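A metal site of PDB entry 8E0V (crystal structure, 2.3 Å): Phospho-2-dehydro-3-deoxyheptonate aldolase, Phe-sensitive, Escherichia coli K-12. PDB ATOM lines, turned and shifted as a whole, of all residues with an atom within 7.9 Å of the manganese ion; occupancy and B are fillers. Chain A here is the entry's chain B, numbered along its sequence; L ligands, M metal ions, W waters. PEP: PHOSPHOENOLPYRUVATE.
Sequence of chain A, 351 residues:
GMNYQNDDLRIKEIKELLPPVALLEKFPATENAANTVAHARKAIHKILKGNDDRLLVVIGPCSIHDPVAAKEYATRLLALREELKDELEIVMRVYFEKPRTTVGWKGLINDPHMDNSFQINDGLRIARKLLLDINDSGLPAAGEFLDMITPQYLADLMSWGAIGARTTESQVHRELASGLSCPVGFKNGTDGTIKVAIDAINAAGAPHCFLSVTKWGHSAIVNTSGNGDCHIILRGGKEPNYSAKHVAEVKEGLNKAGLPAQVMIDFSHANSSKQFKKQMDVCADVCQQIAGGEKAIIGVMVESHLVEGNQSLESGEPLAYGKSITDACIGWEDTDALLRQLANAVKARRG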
ATOM      1  N   GLY A  60     -23.979  24.173 -16.104  1.00  0.00           N
ATOM      2  CA  GLY A  60     -23.724  24.239 -14.689  1.00  0.00           C
ATOM      3  C   GLY A  60     -22.801  23.128 -14.231  1.00  0.00           C
ATOM      4  O   GLY A  60     -22.182  22.432 -15.048  1.00  0.00           O
ATOM      5  N   PRO A  61     -22.689  22.954 -12.914  1.00  0.00           N
ATOM      6  CA  PRO A  61     -21.696  22.023 -12.384  1.00  0.00           C
ATOM      7  C   PRO A  61     -21.959  20.620 -12.875  1.00  0.00           C
ATOM      8  O   PRO A  61     -23.109  20.206 -13.046  1.00  0.00           O
ATOM      9  CB  PRO A  61     -21.891  22.134 -10.860  1.00  0.00           C
ATOM     10  CG  PRO A  61     -22.440  23.534 -10.665  1.00  0.00           C
ATOM     11  CD  PRO A  61     -23.342  23.745 -11.856  1.00  0.00           C
ATOM     12  N   CYS A  62     -20.860  19.889 -13.056  1.00  0.00           N
ATOM     13  CA  CYS A  62     -20.963  18.452 -13.268  1.00  0.00           C
ATOM     14  C   CYS A  62     -21.812  17.820 -12.180  1.00  0.00           C
ATOM     15  O   CYS A  62     -22.706  17.006 -12.463  1.00  0.00           O
ATOM     16  CB  CYS A  62     -19.576  17.822 -13.299  1.00  0.00           C
ATOM     17  SG  CYS A  62     -19.575  16.019 -13.309  1.00  0.00           S
ATOM     18  N   SER A  63     -21.544  18.186 -10.923  1.00  0.00           N
ATOM     19  CA  SER A  63     -22.257  17.654  -9.761  1.00  0.00           C
ATOM     20  C   SER A  63     -22.374  18.766  -8.748  1.00  0.00           C
ATOM     21  O   SER A  63     -21.458  19.580  -8.619  1.00  0.00           O
ATOM     22  CB  SER A  63     -21.524  16.468  -9.129  1.00  0.00           C
ATOM     23  OG  SER A  63     -20.311  16.888  -8.526  1.00  0.00           O
ATOM     24  N   ARG A  93     -27.714  23.159 -14.739  1.00  0.00           N
ATOM     25  CA  ARG A  93     -27.420  21.812 -14.251  1.00  0.00           C
ATOM     26  C   ARG A  93     -27.460  21.763 -12.725  1.00  0.00           C
ATOM     27  O   ARG A  93     -26.660  22.406 -12.034  1.00  0.00           O
ATOM     28  CB  ARG A  93     -26.050  21.351 -14.750  1.00  0.00           C
ATOM     29  CG  ARG A  93     -26.013  21.030 -16.228  1.00  0.00           C
ATOM     30  CD  ARG A  93     -24.630  20.479 -16.628  1.00  0.00           C
ATOM     31  NE  ARG A  93     -24.167  19.404 -15.737  1.00  0.00           N
ATOM     32  CZ  ARG A  93     -24.033  18.141 -16.100  1.00  0.00           C
ATOM     33  NH1 ARG A  93     -24.373  17.727 -17.319  1.00  0.00           N
ATOM     34  NH2 ARG A  93     -23.536  17.257 -15.231  1.00  0.00           N
ATOM     35  N   TYR A  95     -27.240  18.603 -10.783  1.00  0.00           N
ATOM     36  CA  TYR A  95     -27.165  17.147 -10.786  1.00  0.00           C
ATOM     37  C   TYR A  95     -26.870  16.627  -9.386  1.00  0.00           C
ATOM     38  O   TYR A  95     -25.811  16.918  -8.830  1.00  0.00           O
ATOM     39  CB  TYR A  95     -26.109  16.661 -11.789  1.00  0.00           C
ATOM     40  CG  TYR A  95     -26.573  16.675 -13.247  1.00  0.00           C
ATOM     41  CD1 TYR A  95     -27.377  17.707 -13.735  1.00  0.00           C
ATOM     42  CD2 TYR A  95     -26.178  15.682 -14.117  1.00  0.00           C
ATOM     43  CE1 TYR A  95     -27.816  17.722 -15.061  1.00  0.00           C
ATOM     44  CE2 TYR A  95     -26.580  15.704 -15.460  1.00  0.00           C
ATOM     45  CZ  TYR A  95     -27.397  16.715 -15.920  1.00  0.00           C
ATOM     46  OH  TYR A  95     -27.799  16.711 -17.240  1.00  0.00           O
ATOM     47  N   LYS A  98     -24.765  10.832  -9.678  1.00  0.00           N
ATOM     48  CA  LYS A  98     -23.647  10.669 -10.625  1.00  0.00           C
ATOM     49  C   LYS A  98     -23.421   9.187 -10.899  1.00  0.00           C
ATOM     50  O   LYS A  98     -23.249   8.412  -9.949  1.00  0.00           O
ATOM     51  CB  LYS A  98     -22.412  11.369 -10.066  1.00  0.00           C
ATOM     52  CG  LYS A  98     -22.606  12.829  -9.678  1.00  0.00           C
ATOM     53  CD  LYS A  98     -23.028  13.708 -10.842  1.00  0.00           C
ATOM     54  CE  LYS A  98     -22.189  13.495 -12.080  1.00  0.00           C
ATOM     55  NZ  LYS A  98     -22.650  14.342 -13.204  1.00  0.00           N
ATOM     56  N   PRO A  99     -23.436   8.749 -12.172  1.00  0.00           N
ATOM     57  CA  PRO A  99     -23.112   7.349 -12.497  1.00  0.00           C
ATOM     58  C   PRO A  99     -21.596   7.194 -12.584  1.00  0.00           C
ATOM     59  O   PRO A  99     -20.929   8.001 -13.229  1.00  0.00           O
ATOM     60  CB  PRO A  99     -23.779   7.135 -13.861  1.00  0.00           C
ATOM     61  CG  PRO A  99     -23.709   8.524 -14.512  1.00  0.00           C
ATOM     62  CD  PRO A  99     -23.785   9.538 -13.364  1.00  0.00           C
ATOM     63  N   GLU A 144     -29.969  14.736 -14.080  1.00  0.00           N
ATOM     64  CA  GLU A 144     -29.977  13.377 -14.606  1.00  0.00           C
ATOM     65  C   GLU A 144     -30.829  12.489 -13.697  1.00  0.00           C
ATOM     66  O   GLU A 144     -30.645  12.473 -12.470  1.00  0.00           O
ATOM     67  CB  GLU A 144     -28.565  12.772 -14.738  1.00  0.00           C
ATOM     68  CG  GLU A 144     -28.602  11.365 -15.447  1.00  0.00           C
ATOM     69  CD  GLU A 144     -27.271  10.578 -15.448  1.00  0.00           C
ATOM     70  OE1 GLU A 144     -26.200  11.213 -15.338  1.00  0.00           O
ATOM     71  OE2 GLU A 144     -27.304   9.299 -15.586  1.00  0.00           O
ATOM     72  N   ARG A 166     -24.900   5.890 -19.975  1.00  0.00           N
ATOM     73  CA  ARG A 166     -24.738   4.508 -19.487  1.00  0.00           C
ATOM     74  C   ARG A 166     -26.067   3.857 -19.129  1.00  0.00           C
ATOM     75  O   ARG A 166     -26.063   2.684 -18.736  1.00  0.00           O
ATOM     76  CB  ARG A 166     -23.800   4.445 -18.270  1.00  0.00           C
ATOM     77  CG  ARG A 166     -22.337   4.821 -18.539  1.00  0.00           C
ATOM     78  CD  ARG A 166     -21.651   5.365 -17.256  1.00  0.00           C
ATOM     79  NE  ARG A 166     -20.360   5.981 -17.551  1.00  0.00           N
ATOM     80  CZ  ARG A 166     -20.215   7.255 -17.921  1.00  0.00           C
ATOM     81  NH1 ARG A 166     -21.245   8.091 -17.990  1.00  0.00           N
ATOM     82  NH2 ARG A 166     -19.011   7.695 -18.252  1.00  0.00           N
ATOM     83  N   LYS A 187     -28.612  10.529 -23.655  1.00  0.00           N
ATOM     84  CA  LYS A 187     -27.271  10.569 -24.214  1.00  0.00           C
ATOM     85  C   LYS A 187     -27.094   9.423 -25.211  1.00  0.00           C
ATOM     86  O   LYS A 187     -27.749   8.384 -25.112  1.00  0.00           O
ATOM     87  CB  LYS A 187     -26.210  10.461 -23.126  1.00  0.00           C
ATOM     88  CG  LYS A 187     -26.296  11.561 -22.064  1.00  0.00           C
ATOM     89  CD  LYS A 187     -25.835  12.891 -22.607  1.00  0.00           C
ATOM     90  CE  LYS A 187     -25.431  13.867 -21.489  1.00  0.00           C
ATOM     91  NZ  LYS A 187     -23.989  13.761 -21.044  1.00  0.00           N
ATOM     92  N   ASP A 266     -23.840  18.037 -26.261  1.00  0.00           N
ATOM     93  CA  ASP A 266     -23.118  18.147 -25.007  1.00  0.00           C
ATOM     94  C   ASP A 266     -21.677  18.521 -25.340  1.00  0.00           C
ATOM     95  O   ASP A 266     -20.998  17.781 -26.073  1.00  0.00           O
ATOM     96  CB  ASP A 266     -23.168  16.813 -24.254  1.00  0.00           C
ATOM     97  CG  ASP A 266     -22.318  16.800 -23.001  1.00  0.00           C
ATOM     98  OD1 ASP A 266     -21.943  17.910 -22.528  1.00  0.00           O
ATOM     99  OD2 ASP A 266     -22.052  15.699 -22.467  1.00  0.00           O
ATOM    100  N   SER A 268     -19.194  18.678 -23.253  1.00  0.00           N
ATOM    101  CA  SER A 268     -18.246  18.126 -22.290  1.00  0.00           C
ATOM    102  C   SER A 268     -18.087  16.614 -22.514  1.00  0.00           C
ATOM    103  O   SER A 268     -18.356  16.108 -23.598  1.00  0.00           O
ATOM    104  CB  SER A 268     -18.742  18.466 -20.880  1.00  0.00           C
ATOM    105  OG  SER A 268     -17.778  18.075 -19.911  1.00  0.00           O
ATOM    106  N   HIS A 269     -17.617  15.900 -21.483  1.00  0.00           N
ATOM    107  CA  HIS A 269     -17.411  14.433 -21.483  1.00  0.00           C
ATOM    108  C   HIS A 269     -16.581  14.050 -22.701  1.00  0.00           C
ATOM    109  O   HIS A 269     -15.523  14.651 -22.922  1.00  0.00           O
ATOM    110  CB  HIS A 269     -18.763  13.771 -21.353  1.00  0.00           C
ATOM    111  CG  HIS A 269     -19.582  14.331 -20.230  1.00  0.00           C
ATOM    112  ND1 HIS A 269     -20.597  15.246 -20.419  1.00  0.00           N
ATOM    113  CD2 HIS A 269     -19.478  14.168 -18.884  1.00  0.00           C
ATOM    114  CE1 HIS A 269     -21.102  15.605 -19.255  1.00  0.00           C
ATOM    115  NE2 HIS A 269     -20.442  14.953 -18.311  1.00  0.00           N
ATOM    116  N   MET A 301     -25.270  21.588 -23.907  1.00  0.00           N
ATOM    117  CA  MET A 301     -25.025  21.354 -22.496  1.00  0.00           C
ATOM    118  C   MET A 301     -23.551  21.590 -22.248  1.00  0.00           C
ATOM    119  O   MET A 301     -22.710  21.271 -23.095  1.00  0.00           O
ATOM    120  CB  MET A 301     -25.492  19.935 -22.102  1.00  0.00           C
ATOM    121  CG  MET A 301     -24.744  19.203 -20.994  1.00  0.00           C
ATOM    122  SD  MET A 301     -25.305  17.459 -20.672  1.00  0.00           S
ATOM    123  CE  MET A 301     -27.079  17.596 -20.487  1.00  0.00           C
ATOM    124  N   GLU A 303     -20.500  21.902 -18.900  1.00  0.00           N
ATOM    125  CA  GLU A 303     -20.132  21.687 -17.514  1.00  0.00           C
ATOM    126  C   GLU A 303     -19.331  22.893 -17.027  1.00  0.00           C
ATOM    127  O   GLU A 303     -18.157  23.068 -17.384  1.00  0.00           O
ATOM    128  CB  GLU A 303     -19.387  20.362 -17.367  1.00  0.00           C
ATOM    129  CG  GLU A 303     -20.376  19.134 -17.432  1.00  0.00           C
ATOM    130  CD  GLU A 303     -19.722  17.831 -17.042  1.00  0.00           C
ATOM    131  OE1 GLU A 303     -18.548  17.595 -17.457  1.00  0.00           O
ATOM    132  OE2 GLU A 303     -20.388  17.017 -16.354  1.00  0.00           O
ATOM    133  N   SER A 324     -15.339  21.794  -8.988  1.00  0.00           N
ATOM    134  CA  SER A 324     -16.010  20.492  -9.127  1.00  0.00           C
ATOM    135  C   SER A 324     -15.214  19.342  -8.503  1.00  0.00           C
ATOM    136  O   SER A 324     -13.990  19.256  -8.655  1.00  0.00           O
ATOM    137  CB  SER A 324     -16.250  20.167 -10.605  1.00  0.00           C
ATOM    138  OG  SER A 324     -16.728  18.831 -10.800  1.00  0.00           O
ATOM    139  N   THR A 326     -16.144  16.189  -9.328  1.00  0.00           N
ATOM    140  CA  THR A 326     -16.261  15.125 -10.316  1.00  0.00           C
ATOM    141  C   THR A 326     -15.494  15.596 -11.559  1.00  0.00           C
ATOM    142  O   THR A 326     -14.293  15.815 -11.471  1.00  0.00           O
ATOM    143  CB  THR A 326     -17.720  14.751 -10.526  1.00  0.00           C
ATOM    144  OG1 THR A 326     -18.506  15.932 -10.711  1.00  0.00           O
ATOM    145  CG2 THR A 326     -18.252  13.989  -9.291  1.00  0.00           C
ATOM    146  N   ASP A 327     -16.154  15.734 -12.716  1.00  0.00           N
ATOM    147  CA  ASP A 327     -15.417  16.092 -13.931  1.00  0.00           C
ATOM    148  C   ASP A 327     -14.948  17.543 -13.867  1.00  0.00           C
ATOM    149  O   ASP A 327     -15.480  18.352 -13.120  1.00  0.00           O
ATOM    150  CB  ASP A 327     -16.274  15.903 -15.182  1.00  0.00           C
ATOM    151  CG  ASP A 327     -16.775  14.484 -15.349  1.00  0.00           C
ATOM    152  OD1 ASP A 327     -16.085  13.547 -14.873  1.00  0.00           O
ATOM    153  OD2 ASP A 327     -17.850  14.302 -15.975  1.00  0.00           O
ATOM    154  N   ALA A 328     -13.963  17.876 -14.711  1.00  0.00           N
ATOM    155  CA  ALA A 328     -13.482  19.255 -14.736  1.00  0.00           C
ATOM    156  C   ALA A 328     -14.465  20.137 -15.509  1.00  0.00           C
ATOM    157  O   ALA A 328     -15.032  19.718 -16.520  1.00  0.00           O
ATOM    158  CB  ALA A 328     -12.087  19.333 -15.361  1.00  0.00           C
ATOM    159  N   CYS A 329     -14.677  21.349 -14.990  1.00  0.00           N
ATOM    160  CA  CYS A 329     -15.612  22.315 -15.574  1.00  0.00           C
ATOM    161  C   CYS A 329     -14.884  23.571 -16.007  1.00  0.00           C
ATOM    162  O   CYS A 329     -13.824  23.887 -15.474  1.00  0.00           O
ATOM    163  CB  CYS A 329     -16.710  22.708 -14.571  1.00  0.00           C
ATOM    164  SG  CYS A 329     -17.623  21.309 -13.902  1.00  0.00           S
HETATM  165  C1  PEP L   1     -23.528  14.007 -17.358  1.00  0.00           C
HETATM  166  O1  PEP L   1     -23.916  14.708 -18.287  1.00  0.00           O
HETATM  167  O2' PEP L   1     -23.589  14.349 -16.176  1.00  0.00           O
HETATM  168  C2  PEP L   1     -23.048  12.716 -17.667  1.00  0.00           C
HETATM  169  C3  PEP L   1     -22.750  11.691 -16.765  1.00  0.00           C
HETATM  170  O2  PEP L   1     -22.854  12.462 -18.995  1.00  0.00           O
HETATM  171  P   PEP L   1     -22.777  11.028 -19.686  1.00  0.00           P
HETATM  172  O1P PEP L   1     -23.921  10.205 -19.192  1.00  0.00           O
HETATM  173  O2P PEP L   1     -22.879  11.266 -21.156  1.00  0.00           O
HETATM  174  O3P PEP L   1     -21.472  10.404 -19.328  1.00  0.00           O
HETATM  175 MN    MN M   1     -19.741  15.303 -15.926  1.00  0.00          MN
HETATM  176  O   HOH W   1     -19.379  12.171 -15.649  1.00  0.00           O
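NE2 of His 269 lies close to O1 of the ligand (3.5 Å).
The side-chain amino group (NZ) of Lys 98 lies within salt-bridge range of an oxygen (O2') of the ligand, 3.1 Å away.
The guanidinium group (NH2) of Arg 93 lies within salt-bridge range of an oxygen (O2') of the ligand, 3.1 Å away.
The side-chain amino group (NZ) of Lys 187 is in salt-bridge range of an oxygen (O2P) of the ligand.
An oxygen (O3P) of the ligand is in salt-bridge range of the guanidinium group (NH1) of Arg 166 (2.7 Å).
The guanidinium group (NH2) of Arg 93 sits close to the side-chain carboxylate (OE2) of Glu 303, 3.4 Å away.
OE1 of Glu 303 sits at hydrogen-bond distance from OG of Ser 268 (2.6 Å).
The backbone carbonyl oxygen (O) of Asp 327 is in hydrogen-bond range of the side-chain sulfur (SG) of Cys 329 (3.7 Å).
The side-chain hydroxyl (OG) of Ser 324 sits at hydrogen-bond distance from the backbone carbonyl oxygen (O) of Asp 327.
A ring nitrogen (ND1) of His 269 is in hydrogen-bond range of the side-chain carboxylate (OD2) of Asp 266, 2.6 Å away.
NH2 of Arg 93 lies within hydrogen-bond range of O of Cys 62, 2.9 Å away.
The side-chain sulfur of Cys 62 sits close to the side-chain hydroxyl of Thr 326 (2.8 Å).
SG of Cys 329 lies within hydrogen-bond range of N of Cys 62, at 3.6 Å.
Of the 21 residues printed, 4 come within 4 Å of the manganese ion.
The nearest printed residue that does not touch the manganese ion is Lys 98 (4.1 Å).
The manganese ion is bound by OE2 of Glu 303 (1.9 Å), OD2 of Asp 327 (2.1 Å), NE2 of His 269 (2.5 Å) and SG of Cys 62 (2.7 Å).
The manganese ion has four donor atoms within binding distance.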
